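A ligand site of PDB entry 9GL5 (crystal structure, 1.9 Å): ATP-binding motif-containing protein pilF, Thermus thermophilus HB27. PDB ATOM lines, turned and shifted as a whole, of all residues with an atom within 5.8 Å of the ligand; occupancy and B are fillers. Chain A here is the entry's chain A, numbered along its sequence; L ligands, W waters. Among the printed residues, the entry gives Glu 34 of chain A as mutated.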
ATOM      1  N   LEU A  10      -8.220 -26.939  -1.348  1.00  0.00           N
ATOM      2  CA  LEU A  10      -9.059 -25.798  -0.999  1.00  0.00           C
ATOM      3  C   LEU A  10     -10.398 -26.260  -0.426  1.00  0.00           C
ATOM      4  O   LEU A  10     -10.933 -27.297  -0.811  1.00  0.00           O
ATOM      5  CB  LEU A  10      -9.338 -24.908  -2.220  1.00  0.00           C
ATOM      6  CG  LEU A  10      -8.142 -24.385  -3.011  1.00  0.00           C
ATOM      7  CD1 LEU A  10      -8.588 -23.821  -4.353  1.00  0.00           C
ATOM      8  CD2 LEU A  10      -7.368 -23.345  -2.217  1.00  0.00           C
ATOM      9  N   LYS A  11     -10.921 -25.472   0.512  1.00  0.00           N
ATOM     10  CA  LYS A  11     -12.277 -25.683   0.968  1.00  0.00           C
ATOM     11  C   LYS A  11     -13.258 -25.289  -0.132  1.00  0.00           C
ATOM     12  O   LYS A  11     -12.899 -24.622  -1.108  1.00  0.00           O
ATOM     13  CB  LYS A  11     -12.537 -24.896   2.256  1.00  0.00           C
ATOM     14  CG  LYS A  11     -11.603 -25.264   3.402  1.00  0.00           C
ATOM     15  CD  LYS A  11     -11.867 -24.397   4.650  1.00  0.00           C
ATOM     16  CE  LYS A  11     -10.827 -24.656   5.724  1.00  0.00           C
ATOM     17  NZ  LYS A  11     -10.700 -23.495   6.661  1.00  0.00           N
ATOM     18  N   LEU A  12     -14.512 -25.738   0.019  1.00  0.00           N
ATOM     19  CA  LEU A  12     -15.502 -25.483  -1.028  1.00  0.00           C
ATOM     20  C   LEU A  12     -15.643 -23.996  -1.313  1.00  0.00           C
ATOM     21  O   LEU A  12     -15.664 -23.574  -2.481  1.00  0.00           O
ATOM     22  CB  LEU A  12     -16.856 -26.047  -0.609  1.00  0.00           C
ATOM     23  CG  LEU A  12     -18.002 -25.561  -1.492  1.00  0.00           C
ATOM     24  CD1 LEU A  12     -17.862 -26.137  -2.908  1.00  0.00           C
ATOM     25  CD2 LEU A  12     -19.340 -25.941  -0.876  1.00  0.00           C
ATOM     26  N   GLY A  13     -15.747 -23.179  -0.249  1.00  0.00           N
ATOM     27  CA  GLY A  13     -15.942 -21.755  -0.445  1.00  0.00           C
ATOM     28  C   GLY A  13     -14.816 -21.114  -1.234  1.00  0.00           C
ATOM     29  O   GLY A  13     -15.055 -20.374  -2.197  1.00  0.00           O
ATOM     30  N   GLU A  14     -13.573 -21.439  -0.858  1.00  0.00           N
ATOM     31  CA  GLU A  14     -12.410 -20.901  -1.555  1.00  0.00           C
ATOM     32  C   GLU A  14     -12.414 -21.311  -3.020  1.00  0.00           C
ATOM     33  O   GLU A  14     -12.087 -20.518  -3.902  1.00  0.00           O
ATOM     34  CB  GLU A  14     -11.129 -21.364  -0.858  1.00  0.00           C
ATOM     35  CG  GLU A  14     -11.071 -20.979   0.622  1.00  0.00           C
ATOM     36  CD  GLU A  14      -9.951 -21.685   1.395  1.00  0.00           C
ATOM     37  OE1 GLU A  14      -9.675 -22.876   1.110  1.00  0.00           O
ATOM     38  OE2 GLU A  14      -9.359 -21.046   2.290  1.00  0.00           O
ATOM     39  N   LEU A  15     -12.791 -22.564  -3.288  1.00  0.00           N
ATOM     40  CA  LEU A  15     -12.879 -23.084  -4.646  1.00  0.00           C
ATOM     41  C   LEU A  15     -13.837 -22.245  -5.486  1.00  0.00           C
ATOM     42  O   LEU A  15     -13.489 -21.801  -6.588  1.00  0.00           O
ATOM     43  CB  LEU A  15     -13.334 -24.534  -4.610  1.00  0.00           C
ATOM     44  CG  LEU A  15     -12.769 -25.548  -5.606  1.00  0.00           C
ATOM     45  CD1 LEU A  15     -11.356 -25.201  -5.993  1.00  0.00           C
ATOM     46  CD2 LEU A  15     -12.819 -26.918  -4.950  1.00  0.00           C
ATOM     47  N   LEU A  27     -20.011 -15.531   0.243  1.00  0.00           N
ATOM     48  CA  LEU A  27     -19.373 -16.588   1.041  1.00  0.00           C
ATOM     49  C   LEU A  27     -19.423 -16.252   2.532  1.00  0.00           C
ATOM     50  O   LEU A  27     -19.760 -17.095   3.364  1.00  0.00           O
ATOM     51  CB  LEU A  27     -17.940 -16.798   0.578  1.00  0.00           C
ATOM     52  CG  LEU A  27     -17.154 -17.840   1.375  1.00  0.00           C
ATOM     53  CD1 LEU A  27     -17.857 -19.196   1.318  1.00  0.00           C
ATOM     54  CD2 LEU A  27     -15.713 -17.951   0.900  1.00  0.00           C
ATOM     55  N   LEU A  31     -21.154 -18.407   5.395  1.00  0.00           N
ATOM     56  CA  LEU A  31     -20.382 -18.970   6.493  1.00  0.00           C
ATOM     57  C   LEU A  31     -20.863 -18.481   7.854  1.00  0.00           C
ATOM     58  O   LEU A  31     -20.797 -19.223   8.838  1.00  0.00           O
ATOM     59  CB  LEU A  31     -18.901 -18.647   6.304  1.00  0.00           C
ATOM     60  CG  LEU A  31     -18.132 -19.432   5.240  1.00  0.00           C
ATOM     61  CD1 LEU A  31     -16.767 -18.815   5.047  1.00  0.00           C
ATOM     62  CD2 LEU A  31     -18.018 -20.906   5.605  1.00  0.00           C
ATOM     63  N   GLU A  34     -23.935 -20.459   8.426  1.00  0.00           N
ATOM     64  CA  GLU A  34     -23.603 -21.846   8.717  1.00  0.00           C
ATOM     65  C   GLU A  34     -23.162 -22.005  10.170  1.00  0.00           C
ATOM     66  O   GLU A  34     -23.551 -22.967  10.839  1.00  0.00           O
ATOM     67  CB  GLU A  34     -22.510 -22.352   7.789  1.00  0.00           C
ATOM     68  CG  GLU A  34     -21.926 -23.681   8.266  1.00  0.00           C
ATOM     69  CD  GLU A  34     -21.175 -24.424   7.197  1.00  0.00           C
ATOM     70  OE1 GLU A  34     -20.974 -25.649   7.373  1.00  0.00           O
ATOM     71  OE2 GLU A  34     -20.779 -23.802   6.188  1.00  0.00           O
ATOM     72  N   GLY A  38     -25.550 -24.750  11.239  1.00  0.00           N
ATOM     73  CA  GLY A  38     -25.021 -26.077  11.044  1.00  0.00           C
ATOM     74  C   GLY A  38     -25.279 -26.700   9.683  1.00  0.00           C
ATOM     75  O   GLY A  38     -24.767 -27.785   9.412  1.00  0.00           O
ATOM     76  N   ASP A  39     -26.058 -26.042   8.807  1.00  0.00           N
ATOM     77  CA  ASP A  39     -26.347 -26.590   7.488  1.00  0.00           C
ATOM     78  C   ASP A  39     -25.073 -26.700   6.667  1.00  0.00           C
ATOM     79  O   ASP A  39     -24.091 -25.975   6.872  1.00  0.00           O
ATOM     80  CB  ASP A  39     -27.351 -25.705   6.724  1.00  0.00           C
ATOM     81  CG  ASP A  39     -28.793 -25.886   7.196  1.00  0.00           C
ATOM     82  OD1 ASP A  39     -29.048 -26.748   8.066  1.00  0.00           O
ATOM     83  OD2 ASP A  39     -29.671 -25.150   6.695  1.00  0.00           O
ATOM     84  N   LEU A  40     -25.096 -27.631   5.713  1.00  0.00           N
ATOM     85  CA  LEU A  40     -24.016 -27.754   4.741  1.00  0.00           C
ATOM     86  C   LEU A  40     -23.821 -26.441   3.998  1.00  0.00           C
ATOM     87  O   LEU A  40     -24.783 -25.774   3.626  1.00  0.00           O
ATOM     88  CB  LEU A  40     -24.349 -28.845   3.721  1.00  0.00           C
ATOM     89  CG  LEU A  40     -23.922 -30.272   3.993  1.00  0.00           C
ATOM     90  CD1 LEU A  40     -24.289 -31.083   2.757  1.00  0.00           C
ATOM     91  CD2 LEU A  40     -22.439 -30.352   4.310  1.00  0.00           C
ATOM     92  N   LEU A  41     -22.558 -26.086   3.771  1.00  0.00           N
ATOM     93  CA  LEU A  41     -22.241 -24.804   3.128  1.00  0.00           C
ATOM     94  C   LEU A  41     -22.851 -24.727   1.735  1.00  0.00           C
ATOM     95  O   LEU A  41     -23.508 -23.749   1.390  1.00  0.00           O
ATOM     96  CB  LEU A  41     -20.729 -24.602   3.053  1.00  0.00           C
ATOM     97  CG  LEU A  41     -20.345 -23.288   2.380  1.00  0.00           C
ATOM     98  CD1 LEU A  41     -20.927 -22.116   3.153  1.00  0.00           C
ATOM     99  CD2 LEU A  41     -18.839 -23.168   2.243  1.00  0.00           C
ATOM    100  N   GLY A  42     -22.613 -25.763   0.920  1.00  0.00           N
ATOM    101  CA  GLY A  42     -23.194 -25.788  -0.409  1.00  0.00           C
ATOM    102  C   GLY A  42     -24.698 -25.630  -0.406  1.00  0.00           C
ATOM    103  O   GLY A  42     -25.259 -24.914  -1.242  1.00  0.00           O
ATOM    104  N   ARG A  43     -25.371 -26.265   0.560  1.00  0.00           N
ATOM    105  CA  ARG A  43     -26.824 -26.080   0.653  1.00  0.00           C
ATOM    106  C   ARG A  43     -27.181 -24.620   0.882  1.00  0.00           C
ATOM    107  O   ARG A  43     -28.141 -24.118   0.299  1.00  0.00           O
ATOM    108  CB  ARG A  43     -27.401 -26.943   1.776  1.00  0.00           C
ATOM    109  CG  ARG A  43     -28.488 -27.894   1.307  1.00  0.00           C
ATOM    110  CD  ARG A  43     -28.067 -29.352   1.498  1.00  0.00           C
ATOM    111  N   LEU A  55     -22.259 -25.629  -7.797  1.00  0.00           N
ATOM    112  CA  LEU A  55     -21.888 -26.378  -6.601  1.00  0.00           C
ATOM    113  C   LEU A  55     -21.307 -27.744  -6.959  1.00  0.00           C
ATOM    114  O   LEU A  55     -20.239 -28.118  -6.448  1.00  0.00           O
ATOM    115  CB  LEU A  55     -23.119 -26.563  -5.703  1.00  0.00           C
ATOM    116  CG  LEU A  55     -22.886 -27.469  -4.489  1.00  0.00           C
ATOM    117  CD1 LEU A  55     -21.778 -26.895  -3.603  1.00  0.00           C
ATOM    118  CD2 LEU A  55     -24.160 -27.672  -3.692  1.00  0.00           C
ATOM    119  N   TYR A  56     -21.985 -28.494  -7.819  1.00  0.00           N
ATOM    120  CA  TYR A  56     -21.505 -29.857  -8.094  1.00  0.00           C
ATOM    121  C   TYR A  56     -20.206 -29.838  -8.880  1.00  0.00           C
ATOM    122  O   TYR A  56     -19.353 -30.708  -8.655  1.00  0.00           O
ATOM    123  CB  TYR A  56     -22.582 -30.673  -8.825  1.00  0.00           C
ATOM    124  CG  TYR A  56     -23.514 -31.321  -7.844  1.00  0.00           C
ATOM    125  CD1 TYR A  56     -24.309 -30.547  -7.002  1.00  0.00           C
ATOM    126  CD2 TYR A  56     -23.559 -32.711  -7.691  1.00  0.00           C
ATOM    127  CE1 TYR A  56     -25.141 -31.105  -6.070  1.00  0.00           C
ATOM    128  CE2 TYR A  56     -24.401 -33.298  -6.746  1.00  0.00           C
ATOM    129  CZ  TYR A  56     -25.181 -32.486  -5.939  1.00  0.00           C
ATOM    130  OH  TYR A  56     -26.012 -33.034  -5.008  1.00  0.00           O
ATOM    131  N   LEU A  59     -17.563 -29.170  -6.239  1.00  0.00           N
ATOM    132  CA  LEU A  59     -17.440 -30.363  -5.392  1.00  0.00           C
ATOM    133  C   LEU A  59     -16.750 -31.496  -6.135  1.00  0.00           C
ATOM    134  O   LEU A  59     -15.964 -32.261  -5.544  1.00  0.00           O
ATOM    135  CB  LEU A  59     -18.825 -30.801  -4.910  1.00  0.00           C
ATOM    136  CG  LEU A  59     -19.480 -30.006  -3.785  1.00  0.00           C
ATOM    137  CD1 LEU A  59     -20.871 -30.538  -3.500  1.00  0.00           C
ATOM    138  CD2 LEU A  59     -18.623 -30.011  -2.507  1.00  0.00           C
ATOM    139  N   GLN A  62     -13.060 -30.720  -6.270  1.00  0.00           N
ATOM    140  CA  GLN A  62     -12.463 -30.847  -4.936  1.00  0.00           C
ATOM    141  C   GLN A  62     -12.117 -32.305  -4.609  1.00  0.00           C
ATOM    142  O   GLN A  62     -11.076 -32.574  -4.015  1.00  0.00           O
ATOM    143  CB  GLN A  62     -13.395 -30.256  -3.888  1.00  0.00           C
ATOM    144  CG  GLN A  62     -12.850 -30.275  -2.454  1.00  0.00           C
ATOM    145  CD  GLN A  62     -13.869 -29.826  -1.434  1.00  0.00           C
ATOM    146  OE1 GLN A  62     -14.920 -30.457  -1.273  1.00  0.00           O
ATOM    147  NE2 GLN A  62     -13.566 -28.718  -0.728  1.00  0.00           N
ATOM    148  N   LYS A  63     -12.993 -33.246  -4.973  1.00  0.00           N
ATOM    149  CA  LYS A  63     -12.774 -34.662  -4.701  1.00  0.00           C
ATOM    150  C   LYS A  63     -12.135 -35.405  -5.862  1.00  0.00           C
ATOM    151  O   LYS A  63     -12.099 -36.646  -5.846  1.00  0.00           O
ATOM    152  CB  LYS A  63     -14.085 -35.341  -4.306  1.00  0.00           C
ATOM    153  CG  LYS A  63     -14.661 -34.882  -2.969  1.00  0.00           C
ATOM    154  CD  LYS A  63     -14.068 -35.594  -1.746  1.00  0.00           C
ATOM    155  CE  LYS A  63     -14.098 -34.662  -0.515  1.00  0.00           C
ATOM    156  NZ  LYS A  63     -14.445 -35.304   0.803  1.00  0.00           N
ATOM    157  N   SER A 109     -23.592 -39.815  -6.503  1.00  0.00           N
ATOM    158  CA  SER A 109     -24.541 -38.744  -6.248  1.00  0.00           C
ATOM    159  C   SER A 109     -24.015 -37.684  -5.275  1.00  0.00           C
ATOM    160  O   SER A 109     -24.569 -36.579  -5.221  1.00  0.00           O
ATOM    161  CB  SER A 109     -25.827 -39.312  -5.671  1.00  0.00           C
ATOM    162  OG  SER A 109     -25.588 -39.733  -4.338  1.00  0.00           O
ATOM    163  N   ASP A 110     -22.981 -38.000  -4.514  1.00  0.00           N
ATOM    164  CA  ASP A 110     -22.449 -37.160  -3.441  1.00  0.00           C
ATOM    165  C   ASP A 110     -20.962 -37.445  -3.347  1.00  0.00           C
ATOM    166  O   ASP A 110     -20.562 -38.588  -3.063  1.00  0.00           O
ATOM    167  CB  ASP A 110     -23.154 -37.472  -2.107  1.00  0.00           C
ATOM    168  CG  ASP A 110     -22.820 -36.469  -0.984  1.00  0.00           C
ATOM    169  OD1 ASP A 110     -21.739 -35.839  -1.007  1.00  0.00           O
ATOM    170  OD2 ASP A 110     -23.642 -36.325  -0.068  1.00  0.00           O
ATOM    171  N   PRO A 111     -20.112 -36.443  -3.579  1.00  0.00           N
ATOM    172  CA  PRO A 111     -18.659 -36.675  -3.516  1.00  0.00           C
ATOM    173  C   PRO A 111     -18.177 -37.101  -2.141  1.00  0.00           C
ATOM    174  O   PRO A 111     -17.140 -37.771  -2.043  1.00  0.00           O
ATOM    175  CB  PRO A 111     -18.074 -35.316  -3.926  1.00  0.00           C
ATOM    176  CG  PRO A 111     -19.136 -34.342  -3.554  1.00  0.00           C
ATOM    177  CD  PRO A 111     -20.433 -35.015  -3.779  1.00  0.00           C
ATOM    178  N   ARG A 112     -18.911 -36.742  -1.082  1.00  0.00           N
ATOM    179  CA  ARG A 112     -18.512 -37.180   0.265  1.00  0.00           C
ATOM    180  C   ARG A 112     -18.534 -38.693   0.400  1.00  0.00           C
ATOM    181  O   ARG A 112     -17.959 -39.228   1.359  1.00  0.00           O
ATOM    182  CB  ARG A 112     -19.428 -36.560   1.319  1.00  0.00           C
ATOM    183  CG  ARG A 112     -19.269 -35.055   1.467  1.00  0.00           C
ATOM    184  CD  ARG A 112     -20.315 -34.495   2.393  1.00  0.00           C
ATOM    185  NE  ARG A 112     -21.653 -34.706   1.862  1.00  0.00           N
ATOM    186  CZ  ARG A 112     -22.771 -34.545   2.553  1.00  0.00           C
ATOM    187  NH1 ARG A 112     -23.952 -34.754   1.986  1.00  0.00           N
ATOM    188  NH2 ARG A 112     -22.703 -34.155   3.822  1.00  0.00           N
HETATM  189  P1  LIG L   1     -14.787 -28.651   2.833  1.00  0.00           P
HETATM  190  O1  LIG L   1     -14.944 -27.895   1.542  1.00  0.00           O
HETATM  191  O2  LIG L   1     -13.360 -29.054   2.766  1.00  0.00           O
HETATM  192  O3  LIG L   1     -14.982 -27.690   4.134  1.00  0.00           O
HETATM  193  C1  LIG L   1     -14.981 -28.298   5.442  1.00  0.00           C
HETATM  194  C2  LIG L   1     -15.727 -27.277   6.356  1.00  0.00           C
HETATM  195  O4  LIG L   1     -15.129 -26.136   6.212  1.00  0.00           O
HETATM  196  C3  LIG L   1     -17.152 -27.067   5.836  1.00  0.00           C
HETATM  197  O5  LIG L   1     -17.935 -27.885   6.572  1.00  0.00           O
HETATM  198  C4  LIG L   1     -17.435 -25.553   6.116  1.00  0.00           C
HETATM  199  O6  LIG L   1     -18.057 -25.491   7.483  1.00  0.00           O
HETATM  200  C5  LIG L   1     -16.273 -24.989   6.245  1.00  0.00           C
HETATM  201  N1  LIG L   1     -15.772 -24.004   5.313  1.00  0.00           N
HETATM  202  C6  LIG L   1     -16.126 -24.583   4.139  1.00  0.00           C
HETATM  203  N2  LIG L   1     -15.671 -23.785   3.124  1.00  0.00           N
HETATM  204  C7  LIG L   1     -15.019 -22.737   3.683  1.00  0.00           C
HETATM  205  C8  LIG L   1     -14.275 -21.498   3.151  1.00  0.00           C
HETATM  206  O7  LIG L   1     -14.164 -21.270   2.004  1.00  0.00           O
HETATM  207  N3  LIG L   1     -13.691 -20.576   4.052  1.00  0.00           N
HETATM  208  C9  LIG L   1     -13.781 -20.791   5.476  1.00  0.00           C
HETATM  209  N4  LIG L   1     -13.204 -19.887   6.431  1.00  0.00           N
HETATM  210  N5  LIG L   1     -14.477 -21.955   5.963  1.00  0.00           N
HETATM  211  C10 LIG L   1     -15.085 -22.905   5.026  1.00  0.00           C
HETATM  212  P2  LIG L   1     -19.394 -28.331   5.761  1.00  0.00           P
HETATM  213  O8  LIG L   1     -20.257 -27.162   5.324  1.00  0.00           O
HETATM  214  O9  LIG L   1     -20.174 -29.206   6.704  1.00  0.00           O
HETATM  215  O10 LIG L   1     -18.810 -29.293   4.426  1.00  0.00           O
HETATM  216  C11 LIG L   1     -18.395 -30.618   4.725  1.00  0.00           C
HETATM  217  C12 LIG L   1     -17.931 -31.176   3.399  1.00  0.00           C
HETATM  218  O11 LIG L   1     -18.939 -31.537   2.663  1.00  0.00           O
HETATM  219  C13 LIG L   1     -17.129 -30.000   2.526  1.00  0.00           C
HETATM  220  O12 LIG L   1     -15.661 -30.136   2.920  1.00  0.00           O
HETATM  221  C14 LIG L   1     -17.351 -30.211   1.306  1.00  0.00           C
HETATM  222  O13 LIG L   1     -16.457 -31.243   0.681  1.00  0.00           O
HETATM  223  C15 LIG L   1     -18.784 -30.926   1.277  1.00  0.00           C
HETATM  224  N6  LIG L   1     -19.780 -30.070   1.106  1.00  0.00           N
HETATM  225  C16 LIG L   1     -19.978 -28.775   1.504  1.00  0.00           C
HETATM  226  N7  LIG L   1     -21.233 -28.430   1.081  1.00  0.00           N
HETATM  227  C17 LIG L   1     -21.769 -29.482   0.456  1.00  0.00           C
HETATM  228  C18 LIG L   1     -23.126 -29.674  -0.215  1.00  0.00           C
HETATM  229  O14 LIG L   1     -23.910 -28.808  -0.242  1.00  0.00           O
HETATM  230  N8  LIG L   1     -23.446 -30.959  -0.803  1.00  0.00           N
HETATM  231  C19 LIG L   1     -22.473 -32.026  -0.773  1.00  0.00           C
HETATM  232  N9  LIG L   1     -22.785 -33.333  -1.395  1.00  0.00           N
HETATM  233  N10 LIG L   1     -21.172 -31.839  -0.148  1.00  0.00           N
HETATM  234  C20 LIG L   1     -20.867 -30.521   0.486  1.00  0.00           C
HETATM  235  O   HOH W   1     -25.715 -31.807  -1.856  1.00  0.00           O
HETATM  236  O   HOH W   2     -26.508 -29.169  -1.347  1.00  0.00           O
HETATM  237  O   HOH W   3     -21.843 -31.521   7.385  1.00  0.00           O
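The backbone NH of Leu 41 is in hydrogen-bond range of an oxygen (O8) of the ligand (3.0 Å). The backbone NH (N) of Leu 12 sits at hydrogen-bond distance from an oxygen (O1) of the ligand. A nitrogen (N7) of the ligand is in hydrogen-bond range of the backbone NH of Gly 42 (3.0 Å). N of Gly 13 sits close to O7 of the ligand (3.4 Å). The side-chain carboxylate (OE1) of Glu 34 sits at hydrogen-bond distance from an oxygen (O6) of the ligand, at 2.9 Å. The side-chain amide oxygen (OE1) of Gln 62 is in hydrogen-bond range of an oxygen (O13) of the ligand, at 2.6 Å. N of Glu 14 sits at hydrogen-bond distance from O7 of the ligand (2.9 Å). N9 of the ligand is in hydrogen-bond range of OD1 of Asp 110. The backbone NH (N) of Arg 43 lies within hydrogen-bond range of an oxygen (O14) of the ligand.
The guanidinium group (NH1) of Arg 112 is in salt-bridge range of the side-chain carboxylate (OD2) of Asp 110 (2.6 Å). The side-chain amide nitrogen of Gln 62 lies within hydrogen-bond range of the backbone carbonyl oxygen of Leu 10 (3.0 Å). N of Lys 11 is in hydrogen-bond range of OE1 of Glu 14, 2.9 Å away. The backbone NH of Leu 12 sits close to the side-chain amide nitrogen of Gln 62.
Residues that only touch the ligand: Arg 112, Lys 11, Leu 40, Leu 59, Leu 31, Leu 55, Pro 111 and Leu 27. The nearest printed residue that does not touch the ligand is Asp 39 (4.3 Å).
Water W1 lies within hydrogen-bond range of a nitrogen (N8) of the ligand (2.6 Å) and the side-chain hydroxyl (OH) of Tyr 56 (3.4 Å).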
